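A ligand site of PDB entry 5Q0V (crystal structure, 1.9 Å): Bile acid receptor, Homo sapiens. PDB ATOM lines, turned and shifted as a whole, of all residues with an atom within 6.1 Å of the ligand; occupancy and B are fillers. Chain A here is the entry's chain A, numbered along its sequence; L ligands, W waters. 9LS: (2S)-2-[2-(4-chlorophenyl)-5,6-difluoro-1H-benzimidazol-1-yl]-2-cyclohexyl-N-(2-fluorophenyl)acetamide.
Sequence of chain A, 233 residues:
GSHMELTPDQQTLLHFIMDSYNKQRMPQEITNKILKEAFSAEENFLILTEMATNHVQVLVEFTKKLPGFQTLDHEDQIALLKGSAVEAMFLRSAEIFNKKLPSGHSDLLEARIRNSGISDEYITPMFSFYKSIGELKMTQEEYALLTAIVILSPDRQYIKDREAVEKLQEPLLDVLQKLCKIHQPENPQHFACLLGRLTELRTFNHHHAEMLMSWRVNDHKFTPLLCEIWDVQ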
ATOM      1  N   PRO A  27     -26.465  -5.354   6.715  1.00  0.00           N
ATOM      2  CA  PRO A  27     -27.117  -4.027   6.843  1.00  0.00           C
ATOM      3  C   PRO A  27     -28.569  -4.020   6.391  1.00  0.00           C
ATOM      4  O   PRO A  27     -29.414  -3.469   7.111  1.00  0.00           O
ATOM      5  CB  PRO A  27     -26.263  -3.106   5.935  1.00  0.00           C
ATOM      6  CG  PRO A  27     -24.947  -3.778   5.880  1.00  0.00           C
ATOM      7  CD  PRO A  27     -25.232  -5.266   5.909  1.00  0.00           C
ATOM      8  N   ILE A  30     -31.215  -5.179   8.987  1.00  0.00           N
ATOM      9  CA  ILE A  30     -31.431  -4.127   9.974  1.00  0.00           C
ATOM     10  C   ILE A  30     -32.345  -2.996   9.454  1.00  0.00           C
ATOM     11  O   ILE A  30     -33.343  -2.686  10.098  1.00  0.00           O
ATOM     12  CB  ILE A  30     -30.034  -3.630  10.469  1.00  0.00           C
ATOM     13  CG1 ILE A  30     -29.214  -4.827  11.041  1.00  0.00           C
ATOM     14  CG2 ILE A  30     -30.145  -2.476  11.475  1.00  0.00           C
ATOM     15  CD1 ILE A  30     -27.715  -4.783  10.853  1.00  0.00           C
ATOM     16  N   THR A  31     -31.999  -2.407   8.289  1.00  0.00           N
ATOM     17  CA  THR A  31     -32.772  -1.297   7.701  1.00  0.00           C
ATOM     18  C   THR A  31     -34.156  -1.746   7.229  1.00  0.00           C
ATOM     19  O   THR A  31     -35.093  -0.956   7.320  1.00  0.00           O
ATOM     20  CB  THR A  31     -31.988  -0.570   6.607  1.00  0.00           C
ATOM     21  OG1 THR A  31     -31.617  -1.490   5.582  1.00  0.00           O
ATOM     22  CG2 THR A  31     -30.763   0.147   7.152  1.00  0.00           C
ATOM     23  N   ILE A  34     -36.437  -1.572  10.366  1.00  0.00           N
ATOM     24  CA  ILE A  34     -36.712  -0.180  10.732  1.00  0.00           C
ATOM     25  C   ILE A  34     -37.666   0.477   9.725  1.00  0.00           C
ATOM     26  O   ILE A  34     -38.579   1.187  10.140  1.00  0.00           O
ATOM     27  CB  ILE A  34     -35.386   0.638  10.911  1.00  0.00           C
ATOM     28  CG1 ILE A  34     -34.459  -0.021  11.951  1.00  0.00           C
ATOM     29  CG2 ILE A  34     -35.676   2.109  11.284  1.00  0.00           C
ATOM     30  CD1 ILE A  34     -32.978   0.442  11.920  1.00  0.00           C
ATOM     31  N   ASN A  44     -38.326  -0.160  20.286  1.00  0.00           N
ATOM     32  CA  ASN A  44     -37.033   0.249  19.729  1.00  0.00           C
ATOM     33  C   ASN A  44     -35.877   0.065  20.726  1.00  0.00           C
ATOM     34  O   ASN A  44     -34.774  -0.265  20.301  1.00  0.00           O
ATOM     35  CB  ASN A  44     -37.075   1.691  19.234  1.00  0.00           C
ATOM     36  CG  ASN A  44     -37.767   1.864  17.903  1.00  0.00           C
ATOM     37  OD1 ASN A  44     -37.595   1.061  16.988  1.00  0.00           O
ATOM     38  ND2 ASN A  44     -38.534   2.928  17.745  1.00  0.00           N
ATOM     39  N   PHE A  45     -36.143   0.271  22.029  1.00  0.00           N
ATOM     40  CA  PHE A  45     -35.116   0.087  23.069  1.00  0.00           C
ATOM     41  C   PHE A  45     -34.695  -1.388  23.129  1.00  0.00           C
ATOM     42  O   PHE A  45     -33.496  -1.676  23.204  1.00  0.00           O
ATOM     43  CB  PHE A  45     -35.599   0.590  24.443  1.00  0.00           C
ATOM     44  CG  PHE A  45     -34.522   0.474  25.507  1.00  0.00           C
ATOM     45  CD1 PHE A  45     -33.506   1.426  25.599  1.00  0.00           C
ATOM     46  CD2 PHE A  45     -34.499  -0.602  26.382  1.00  0.00           C
ATOM     47  CE1 PHE A  45     -32.498   1.301  26.557  1.00  0.00           C
ATOM     48  CE2 PHE A  45     -33.481  -0.721  27.348  1.00  0.00           C
ATOM     49  CZ  PHE A  45     -32.498   0.239  27.426  1.00  0.00           C
ATOM     50  N   ILE A  47     -35.081  -3.591  20.589  1.00  0.00           N
ATOM     51  CA  ILE A  47     -34.436  -3.851  19.291  1.00  0.00           C
ATOM     52  C   ILE A  47     -32.951  -3.480  19.447  1.00  0.00           C
ATOM     53  O   ILE A  47     -32.102  -4.295  19.104  1.00  0.00           O
ATOM     54  CB  ILE A  47     -35.137  -3.101  18.111  1.00  0.00           C
ATOM     55  CG1 ILE A  47     -36.543  -3.712  17.835  1.00  0.00           C
ATOM     56  CG2 ILE A  47     -34.267  -3.144  16.824  1.00  0.00           C
ATOM     57  CD1 ILE A  47     -37.483  -2.848  16.998  1.00  0.00           C
ATOM     58  N   LEU A  48     -32.661  -2.309  20.041  1.00  0.00           N
ATOM     59  CA  LEU A  48     -31.292  -1.840  20.272  1.00  0.00           C
ATOM     60  C   LEU A  48     -30.476  -2.785  21.146  1.00  0.00           C
ATOM     61  O   LEU A  48     -29.330  -3.099  20.781  1.00  0.00           O
ATOM     62  CB  LEU A  48     -31.271  -0.407  20.840  1.00  0.00           C
ATOM     63  CG  LEU A  48     -29.886   0.192  21.199  1.00  0.00           C
ATOM     64  CD1 LEU A  48     -29.039   0.435  19.955  1.00  0.00           C
ATOM     65  CD2 LEU A  48     -30.051   1.463  21.974  1.00  0.00           C
ATOM     66  N   MET A  51     -29.752  -5.979  19.228  1.00  0.00           N
ATOM     67  CA  MET A  51     -28.773  -5.653  18.167  1.00  0.00           C
ATOM     68  C   MET A  51     -27.376  -5.479  18.745  1.00  0.00           C
ATOM     69  O   MET A  51     -26.406  -5.971  18.186  1.00  0.00           O
ATOM     70  CB  MET A  51     -29.166  -4.345  17.446  1.00  0.00           C
ATOM     71  CG  MET A  51     -30.244  -4.518  16.417  1.00  0.00           C
ATOM     72  SD  MET A  51     -29.715  -5.367  14.907  1.00  0.00           S
ATOM     73  CE  MET A  51     -28.449  -4.364  14.448  1.00  0.00           C
ATOM     74  N   ALA A  52     -27.270  -4.747  19.872  1.00  0.00           N
ATOM     75  CA  ALA A  52     -26.001  -4.464  20.531  1.00  0.00           C
ATOM     76  C   ALA A  52     -25.395  -5.700  21.154  1.00  0.00           C
ATOM     77  O   ALA A  52     -24.177  -5.825  21.109  1.00  0.00           O
ATOM     78  CB  ALA A  52     -26.197  -3.386  21.562  1.00  0.00           C
ATOM     79  N   HIS A  55     -24.046  -7.716  18.272  1.00  0.00           N
ATOM     80  CA  HIS A  55     -22.896  -6.976  17.770  1.00  0.00           C
ATOM     81  C   HIS A  55     -21.653  -7.256  18.613  1.00  0.00           C
ATOM     82  O   HIS A  55     -20.607  -7.573  18.028  1.00  0.00           O
ATOM     83  CB  HIS A  55     -23.171  -5.467  17.706  1.00  0.00           C
ATOM     84  CG  HIS A  55     -21.984  -4.681  17.259  1.00  0.00           C
ATOM     85  ND1 HIS A  55     -21.149  -4.059  18.166  1.00  0.00           N
ATOM     86  CD2 HIS A  55     -21.485  -4.492  16.005  1.00  0.00           C
ATOM     87  CE1 HIS A  55     -20.175  -3.505  17.451  1.00  0.00           C
ATOM     88  NE2 HIS A  55     -20.332  -3.744  16.149  1.00  0.00           N
ATOM     89  N   MET A  89     -19.684  -0.212  17.554  1.00  0.00           N
ATOM     90  CA  MET A  89     -21.142  -0.191  17.304  1.00  0.00           C
ATOM     91  C   MET A  89     -21.570   1.058  16.522  1.00  0.00           C
ATOM     92  O   MET A  89     -22.386   0.954  15.606  1.00  0.00           O
ATOM     93  CB  MET A  89     -21.946  -0.310  18.623  1.00  0.00           C
ATOM     94  CG  MET A  89     -23.450   0.006  18.401  1.00  0.00           C
ATOM     95  SD  MET A  89     -24.470   0.159  19.856  1.00  0.00           S
ATOM     96  CE  MET A  89     -23.693   1.612  20.586  1.00  0.00           C
ATOM     97  N   PHE A  90     -21.052   2.221  16.911  1.00  0.00           N
ATOM     98  CA  PHE A  90     -21.360   3.472  16.217  1.00  0.00           C
ATOM     99  C   PHE A  90     -20.756   3.485  14.824  1.00  0.00           C
ATOM    100  O   PHE A  90     -21.386   3.993  13.911  1.00  0.00           O
ATOM    101  CB  PHE A  90     -20.951   4.703  17.025  1.00  0.00           C
ATOM    102  CG  PHE A  90     -21.939   5.007  18.135  1.00  0.00           C
ATOM    103  CD1 PHE A  90     -23.207   5.495  17.845  1.00  0.00           C
ATOM    104  CD2 PHE A  90     -21.608   4.787  19.452  1.00  0.00           C
ATOM    105  CE1 PHE A  90     -24.124   5.767  18.871  1.00  0.00           C
ATOM    106  CE2 PHE A  90     -22.517   5.073  20.483  1.00  0.00           C
ATOM    107  CZ  PHE A  90     -23.767   5.570  20.178  1.00  0.00           C
ATOM    108  N   ARG A  92     -20.238   0.778  12.943  1.00  0.00           N
ATOM    109  CA  ARG A  92     -21.074  -0.141  12.175  1.00  0.00           C
ATOM    110  C   ARG A  92     -22.438   0.507  11.843  1.00  0.00           C
ATOM    111  O   ARG A  92     -22.919   0.377  10.721  1.00  0.00           O
ATOM    112  CB  ARG A  92     -21.234  -1.485  12.909  1.00  0.00           C
ATOM    113  CG  ARG A  92     -22.090  -2.505  12.154  1.00  0.00           C
ATOM    114  CD  ARG A  92     -21.565  -2.820  10.749  1.00  0.00           C
ATOM    115  NE  ARG A  92     -22.281  -3.947  10.177  1.00  0.00           N
ATOM    116  CZ  ARG A  92     -21.989  -4.527   9.026  1.00  0.00           C
ATOM    117  NH1 ARG A  92     -21.000  -4.069   8.267  1.00  0.00           N
ATOM    118  NH2 ARG A  92     -22.686  -5.578   8.606  1.00  0.00           N
ATOM    119  N   SER A  93     -23.016   1.258  12.803  1.00  0.00           N
ATOM    120  CA  SER A  93     -24.276   1.999  12.594  1.00  0.00           C
ATOM    121  C   SER A  93     -24.099   3.050  11.488  1.00  0.00           C
ATOM    122  O   SER A  93     -24.992   3.212  10.647  1.00  0.00           O
ATOM    123  CB  SER A  93     -24.741   2.641  13.892  1.00  0.00           C
ATOM    124  OG  SER A  93     -25.094   1.630  14.834  1.00  0.00           O
ATOM    125  N   ALA A  94     -22.930   3.749  11.468  1.00  0.00           N
ATOM    126  CA  ALA A  94     -22.582   4.743  10.445  1.00  0.00           C
ATOM    127  C   ALA A  94     -22.479   4.093   9.072  1.00  0.00           C
ATOM    128  O   ALA A  94     -23.007   4.632   8.101  1.00  0.00           O
ATOM    129  CB  ALA A  94     -21.276   5.428  10.785  1.00  0.00           C
ATOM    130  N   ILE A  96     -23.978   1.273   8.102  1.00  0.00           N
ATOM    131  CA  ILE A  96     -25.343   0.879   7.738  1.00  0.00           C
ATOM    132  C   ILE A  96     -26.119   2.112   7.269  1.00  0.00           C
ATOM    133  O   ILE A  96     -26.761   2.057   6.222  1.00  0.00           O
ATOM    134  CB  ILE A  96     -26.032   0.118   8.904  1.00  0.00           C
ATOM    135  CG1 ILE A  96     -25.382  -1.251   9.147  1.00  0.00           C
ATOM    136  CG2 ILE A  96     -27.536  -0.044   8.650  1.00  0.00           C
ATOM    137  CD1 ILE A  96     -25.594  -1.803  10.516  1.00  0.00           C
ATOM    138  N   PHE A  97     -26.032   3.233   8.006  1.00  0.00           N
ATOM    139  CA  PHE A  97     -26.758   4.463   7.650  1.00  0.00           C
ATOM    140  C   PHE A  97     -26.359   4.993   6.259  1.00  0.00           C
ATOM    141  O   PHE A  97     -27.193   5.535   5.549  1.00  0.00           O
ATOM    142  CB  PHE A  97     -26.598   5.567   8.725  1.00  0.00           C
ATOM    143  CG  PHE A  97     -27.413   6.806   8.409  1.00  0.00           C
ATOM    144  CD1 PHE A  97     -28.795   6.759   8.411  1.00  0.00           C
ATOM    145  CD2 PHE A  97     -26.792   7.982   7.998  1.00  0.00           C
ATOM    146  CE1 PHE A  97     -29.552   7.875   8.020  1.00  0.00           C
ATOM    147  CE2 PHE A  97     -27.537   9.107   7.646  1.00  0.00           C
ATOM    148  CZ  PHE A  97     -28.915   9.043   7.657  1.00  0.00           C
ATOM    149  N   ASN A  98     -25.097   4.819   5.895  1.00  0.00           N
ATOM    150  CA  ASN A  98     -24.587   5.366   4.651  1.00  0.00           C
ATOM    151  C   ASN A  98     -24.725   4.449   3.433  1.00  0.00           C
ATOM    152  O   ASN A  98     -24.387   4.897   2.334  1.00  0.00           O
ATOM    153  CB  ASN A  98     -23.144   5.814   4.848  1.00  0.00           C
ATOM    154  CG  ASN A  98     -23.105   7.092   5.632  1.00  0.00           C
ATOM    155  OD1 ASN A  98     -23.616   8.134   5.200  1.00  0.00           O
ATOM    156  ND2 ASN A  98     -22.563   7.049   6.836  1.00  0.00           N
ATOM    157  N   LEU A 109     -35.562   6.251   7.085  1.00  0.00           N
ATOM    158  CA  LEU A 109     -34.682   5.586   8.040  1.00  0.00           C
ATOM    159  C   LEU A 109     -34.187   6.588   9.087  1.00  0.00           C
ATOM    160  O   LEU A 109     -34.272   6.300  10.280  1.00  0.00           O
ATOM    161  CB  LEU A 109     -33.502   4.936   7.301  1.00  0.00           C
ATOM    162  CG  LEU A 109     -32.474   4.211   8.174  1.00  0.00           C
ATOM    163  CD1 LEU A 109     -33.051   2.892   8.762  1.00  0.00           C
ATOM    164  CD2 LEU A 109     -31.245   3.915   7.393  1.00  0.00           C
ATOM    165  N   ARG A 112     -37.166   7.717  11.313  1.00  0.00           N
ATOM    166  CA  ARG A 112     -37.524   6.620  12.218  1.00  0.00           C
ATOM    167  C   ARG A 112     -36.526   6.539  13.398  1.00  0.00           C
ATOM    168  O   ARG A 112     -36.967   6.471  14.541  1.00  0.00           O
ATOM    169  CB  ARG A 112     -37.629   5.277  11.475  1.00  0.00           C
ATOM    170  CG  ARG A 112     -38.888   5.154  10.598  1.00  0.00           C
ATOM    171  CD  ARG A 112     -40.017   4.372  11.242  1.00  0.00           C
ATOM    172  NE  ARG A 112     -41.263   4.431  10.457  1.00  0.00           N
ATOM    173  CZ  ARG A 112     -41.538   3.621   9.442  1.00  0.00           C
ATOM    174  NH1 ARG A 112     -42.692   3.738   8.785  1.00  0.00           N
ATOM    175  NH2 ARG A 112     -40.664   2.711   9.054  1.00  0.00           N
ATOM    176  N   ILE A 113     -35.216   6.618  13.115  1.00  0.00           N
ATOM    177  CA  ILE A 113     -34.168   6.593  14.170  1.00  0.00           C
ATOM    178  C   ILE A 113     -34.297   7.839  15.067  1.00  0.00           C
ATOM    179  O   ILE A 113     -34.221   7.727  16.289  1.00  0.00           O
ATOM    180  CB  ILE A 113     -32.753   6.464  13.555  1.00  0.00           C
ATOM    181  CG1 ILE A 113     -32.595   5.131  12.797  1.00  0.00           C
ATOM    182  CG2 ILE A 113     -31.645   6.609  14.630  1.00  0.00           C
ATOM    183  CD1 ILE A 113     -31.468   5.097  11.783  1.00  0.00           C
ATOM    184  N   SER A 116     -36.962   7.221  17.622  1.00  0.00           N
ATOM    185  CA  SER A 116     -36.839   5.895  18.250  1.00  0.00           C
ATOM    186  C   SER A 116     -36.950   5.886  19.787  1.00  0.00           C
ATOM    187  O   SER A 116     -37.180   4.817  20.349  1.00  0.00           O
ATOM    188  CB  SER A 116     -35.544   5.211  17.815  1.00  0.00           C
ATOM    189  OG  SER A 116     -34.403   5.913  18.301  1.00  0.00           O
ATOM    190  N   ILE A 118     -34.533   7.935  21.683  1.00  0.00           N
ATOM    191  CA  ILE A 118     -33.288   8.621  22.033  1.00  0.00           C
ATOM    192  C   ILE A 118     -33.560  10.150  22.158  1.00  0.00           C
ATOM    193  O   ILE A 118     -34.384  10.673  21.403  1.00  0.00           O
ATOM    194  CB  ILE A 118     -32.191   8.262  20.993  1.00  0.00           C
ATOM    195  CG1 ILE A 118     -30.816   8.864  21.361  1.00  0.00           C
ATOM    196  CG2 ILE A 118     -32.612   8.620  19.556  1.00  0.00           C
ATOM    197  CD1 ILE A 118     -29.633   8.180  20.694  1.00  0.00           C
ATOM    198  N   MET A 126     -24.883  12.339  16.891  1.00  0.00           N
ATOM    199  CA  MET A 126     -24.969  11.042  16.236  1.00  0.00           C
ATOM    200  C   MET A 126     -25.101  11.140  14.700  1.00  0.00           C
ATOM    201  O   MET A 126     -24.255  10.597  13.999  1.00  0.00           O
ATOM    202  CB  MET A 126     -26.087  10.194  16.855  1.00  0.00           C
ATOM    203  CG  MET A 126     -26.036   8.732  16.455  1.00  0.00           C
ATOM    204  SD  MET A 126     -27.509   7.828  16.988  1.00  0.00           S
ATOM    205  CE  MET A 126     -28.729   8.521  15.952  1.00  0.00           C
ATOM    206  N   PHE A 127     -26.135  11.851  14.187  1.00  0.00           N
ATOM    207  CA  PHE A 127     -26.349  12.040  12.742  1.00  0.00           C
ATOM    208  C   PHE A 127     -25.256  12.906  12.103  1.00  0.00           C
ATOM    209  O   PHE A 127     -24.935  12.683  10.929  1.00  0.00           O
ATOM    210  CB  PHE A 127     -27.776  12.535  12.403  1.00  0.00           C
ATOM    211  CG  PHE A 127     -28.727  11.354  12.296  1.00  0.00           C
ATOM    212  CD1 PHE A 127     -28.574  10.404  11.294  1.00  0.00           C
ATOM    213  CD2 PHE A 127     -29.723  11.162  13.240  1.00  0.00           C
ATOM    214  CE1 PHE A 127     -29.411   9.285  11.236  1.00  0.00           C
ATOM    215  CE2 PHE A 127     -30.573  10.054  13.166  1.00  0.00           C
ATOM    216  CZ  PHE A 127     -30.401   9.116  12.180  1.00  0.00           C
ATOM    217  N   TYR A 130     -22.559  10.353  11.519  1.00  0.00           N
ATOM    218  CA  TYR A 130     -22.978   9.497  10.382  1.00  0.00           C
ATOM    219  C   TYR A 130     -22.794  10.202   9.041  1.00  0.00           C
ATOM    220  O   TYR A 130     -22.305   9.594   8.091  1.00  0.00           O
ATOM    221  CB  TYR A 130     -24.449   9.035  10.533  1.00  0.00           C
ATOM    222  CG  TYR A 130     -24.762   8.129  11.703  1.00  0.00           C
ATOM    223  CD1 TYR A 130     -23.750   7.529  12.440  1.00  0.00           C
ATOM    224  CD2 TYR A 130     -26.078   7.850  12.045  1.00  0.00           C
ATOM    225  CE1 TYR A 130     -24.032   6.678  13.496  1.00  0.00           C
ATOM    226  CE2 TYR A 130     -26.383   7.017  13.126  1.00  0.00           C
ATOM    227  CZ  TYR A 130     -25.353   6.422  13.839  1.00  0.00           C
ATOM    228  OH  TYR A 130     -25.623   5.618  14.917  1.00  0.00           O
ATOM    229  N   HIS A 208     -22.201   7.558  26.299  1.00  0.00           N
ATOM    230  CA  HIS A 208     -23.004   6.385  25.914  1.00  0.00           C
ATOM    231  C   HIS A 208     -23.979   5.958  27.022  1.00  0.00           C
ATOM    232  O   HIS A 208     -25.120   5.641  26.710  1.00  0.00           O
ATOM    233  CB  HIS A 208     -22.145   5.189  25.405  1.00  0.00           C
ATOM    234  CG  HIS A 208     -21.535   4.335  26.479  1.00  0.00           C
ATOM    235  ND1 HIS A 208     -20.249   4.551  26.938  1.00  0.00           N
ATOM    236  CD2 HIS A 208     -22.044   3.259  27.120  1.00  0.00           C
ATOM    237  CE1 HIS A 208     -20.038   3.633  27.863  1.00  0.00           C
ATOM    238  NE2 HIS A 208     -21.096   2.846  28.024  1.00  0.00           N
ATOM    239  N   MET A 211     -26.854   8.420  27.117  1.00  0.00           N
ATOM    240  CA  MET A 211     -27.583   8.246  25.859  1.00  0.00           C
ATOM    241  C   MET A 211     -28.630   7.142  26.013  1.00  0.00           C
ATOM    242  O   MET A 211     -29.773   7.308  25.598  1.00  0.00           O
ATOM    243  CB  MET A 211     -26.590   7.861  24.743  1.00  0.00           C
ATOM    244  CG  MET A 211     -26.967   8.339  23.371  1.00  0.00           C
ATOM    245  SD  MET A 211     -25.704   8.063  22.084  1.00  0.00           S
ATOM    246  CE  MET A 211     -24.355   9.019  22.717  1.00  0.00           C
ATOM    247  N   LEU A 212     -28.239   6.019  26.648  1.00  0.00           N
ATOM    248  CA  LEU A 212     -29.108   4.879  26.876  1.00  0.00           C
ATOM    249  C   LEU A 212     -30.073   5.086  28.031  1.00  0.00           C
ATOM    250  O   LEU A 212     -31.218   4.670  27.920  1.00  0.00           O
ATOM    251  CB  LEU A 212     -28.285   3.626  27.133  1.00  0.00           C
ATOM    252  CG  LEU A 212     -27.303   3.210  26.053  1.00  0.00           C
ATOM    253  CD1 LEU A 212     -26.159   2.499  26.655  1.00  0.00           C
ATOM    254  CD2 LEU A 212     -27.992   2.398  24.981  1.00  0.00           C
ATOM    255  N   TRP A 215     -33.156   7.243  27.263  1.00  0.00           N
ATOM    256  CA  TRP A 215     -34.093   6.732  26.260  1.00  0.00           C
ATOM    257  C   TRP A 215     -35.491   6.870  26.860  1.00  0.00           C
ATOM    258  O   TRP A 215     -35.670   6.586  28.039  1.00  0.00           O
ATOM    259  CB  TRP A 215     -33.789   5.270  25.949  1.00  0.00           C
ATOM    260  CG  TRP A 215     -34.293   4.810  24.616  1.00  0.00           C
ATOM    261  CD1 TRP A 215     -35.564   4.427  24.301  1.00  0.00           C
ATOM    262  CD2 TRP A 215     -33.522   4.681  23.412  1.00  0.00           C
ATOM    263  NE1 TRP A 215     -35.633   4.043  22.980  1.00  0.00           N
ATOM    264  CE2 TRP A 215     -34.393   4.196  22.408  1.00  0.00           C
ATOM    265  CE3 TRP A 215     -32.173   4.906  23.084  1.00  0.00           C
ATOM    266  CZ2 TRP A 215     -33.968   3.958  21.099  1.00  0.00           C
ATOM    267  CZ3 TRP A 215     -31.748   4.672  21.784  1.00  0.00           C
ATOM    268  CH2 TRP A 215     -32.638   4.196  20.808  1.00  0.00           C
HETATM  269  N1  9LS L   1     -29.068   2.297  15.250  1.00  0.00           N
HETATM  270  N3  9LS L   1     -27.881   4.114  14.688  1.00  0.00           N
HETATM  271  C4  9LS L   1     -29.047   2.315  13.874  1.00  0.00           C
HETATM  272  C5  9LS L   1     -28.312   3.457  13.524  1.00  0.00           C
HETATM  273  C6  9LS L   1     -29.033  -0.080  15.992  1.00  0.00           C
HETATM  274  C7  9LS L   1     -29.731   1.287  16.157  1.00  0.00           C
HETATM  275  C8  9LS L   1     -29.613   1.459  12.934  1.00  0.00           C
HETATM  276  C10 9LS L   1     -28.119   3.753  12.174  1.00  0.00           C
HETATM  277  C13 9LS L   1     -28.683   2.889  11.238  1.00  0.00           C
HETATM  278  C17 9LS L   1     -31.262   1.257  16.007  1.00  0.00           C
HETATM  279  C22 9LS L   1     -27.689   4.192  19.814  1.00  0.00           C
HETATM  280  C24 9LS L   1     -28.771   4.783  19.191  1.00  0.00           C
HETATM  281  C28 9LS L   1     -25.480  -2.455  14.118  1.00  0.00           C
HETATM  282  F23 9LS L   1     -26.895  -0.749  13.272  1.00  0.00           F
HETATM  283  C16 9LS L   1     -26.372  -1.424  14.339  1.00  0.00           C
HETATM  284  C32 9LS L   1     -24.965  -3.128  15.218  1.00  0.00           C
HETATM  285  C31 9LS L   1     -25.346  -2.766  16.503  1.00  0.00           C
HETATM  286  C27 9LS L   1     -26.249  -1.733  16.711  1.00  0.00           C
HETATM  287  C14 9LS L   1     -26.778  -1.039  15.614  1.00  0.00           C
HETATM  288  N9  9LS L   1     -27.700   0.019  15.789  1.00  0.00           N
HETATM  289  O15 9LS L   1     -29.647  -1.141  16.041  1.00  0.00           O
HETATM  290  C29 9LS L   1     -31.929   0.550  17.204  1.00  0.00           C
HETATM  291  C33 9LS L   1     -33.473   0.549  17.096  1.00  0.00           C
HETATM  292  C35 9LS L   1     -34.012   1.971  16.960  1.00  0.00           C
HETATM  293  C34 9LS L   1     -33.379   2.695  15.767  1.00  0.00           C
HETATM  294  C30 9LS L   1     -31.843   2.681  15.871  1.00  0.00           C
HETATM  295  C2  9LS L   1     -28.358   3.392  15.683  1.00  0.00           C
HETATM  296  F21 9LS L   1     -28.517   3.133   9.935  1.00  0.00           F
HETATM  297  C11 9LS L   1     -29.411   1.775  11.620  1.00  0.00           C
HETATM  298  F20 9LS L   1     -29.927   0.970  10.667  1.00  0.00           F
HETATM  299  C12 9LS L   1     -28.153   3.703  17.116  1.00  0.00           C
HETATM  300  C18 9LS L   1     -27.069   3.116  17.771  1.00  0.00           C
HETATM  301  C25 9LS L   1     -26.827   3.364  19.124  1.00  0.00           C
HETATM  302 CL26 9LS L   1     -27.389   4.499  21.504  1.00  0.00          CL
HETATM  303  C19 9LS L   1     -29.001   4.528  17.841  1.00  0.00           C
HETATM  304  O   HOH W   1     -23.948  -6.163  13.977  1.00  0.00           O
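OH of Tyr 130 sits at hydrogen-bond distance from N3 of the ligand. OG of Ser 93 is in hydrogen-bond range of N9 of the ligand, 3.2 Å away.
SD of Met 126 sits close to OH of Tyr 130. The side-chain amide nitrogen (ND2) of Asn 98 lies within hydrogen-bond range of the backbone carbonyl oxygen (O) of Tyr 130 (2.8 Å). OG of Ser 93 lies within hydrogen-bond range of O of Met 89 (2.9 Å). O of Ile 34 sits at hydrogen-bond distance from NH2 of Arg 112, at 2.8 Å. ND2 of Asn 44 lies close to O of Ser 116, 3.5 Å away. The backbone carbonyl oxygen (O) of Ile 113 lies within hydrogen-bond range of the side-chain hydroxyl (OG) of Ser 116, 2.7 Å away. The backbone carbonyl oxygen (O) of Ser 116 sits at hydrogen-bond distance from the indole nitrogen (NE1) of Trp 215, at 3.1 Å. The side-chain hydroxyl of Thr 31 is in hydrogen-bond range of the backbone carbonyl oxygen of Pro 27 (3.3 Å).
N of Phe 97 sits close to F21 of the ligand (3.1 Å). Ile 30 touches the ligand (CG2 to F20, 3.5 Å). Thr 31 touches the ligand (CG2 to F20, 3.7 Å). Ile 34 touches the ligand. O of Asn 44 touches C33 of the ligand, 3.6 Å away. Ile 47 touches the ligand (CG2 to C33, 3.8 Å). Leu 48 touches the ligand. CG of Met 51 touches O15 of the ligand, 3.4 Å away. CB of His 55 touches C31 of the ligand (3.7 Å). Met 89 touches the ligand (CG to C27, 3.7 Å). CE1 of Phe 90 touches C25 of the ligand, 3.6 Å away. Arg 92 touches the ligand. Ile 96 touches the ligand (CD1 to F23, 3.2 Å). Leu 109 touches the ligand (CD2 to F21, 3.8 Å). Ile 113 touches the ligand (CD1 to C13, 3.6 Å). CB of Ser 116 touches C35 of the ligand, at 3.7 Å. Ile 118 touches the ligand (CD1 to C24, 3.8 Å). SD of Met 126 touches C19 of the ligand, 3.7 Å away. Met 211 touches the ligand (SD to CL26, 3.98 Å). Trp 215 touches the ligand. Within 4 Å of the ligand: Ile 30, Thr 31, Ile 34, Asn 44, Ile 47, Leu 48, Met 51, His 55, Met 89, Phe 90, Arg 92, Ser 93, Ile 96, Phe 97, Leu 109, Ile 113, Ser 116, Ile 118, Met 126, Tyr 130, Met 211 and Trp 215. The nearest printed residue that does not touch the ligand is Leu 212 (4.1 Å).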
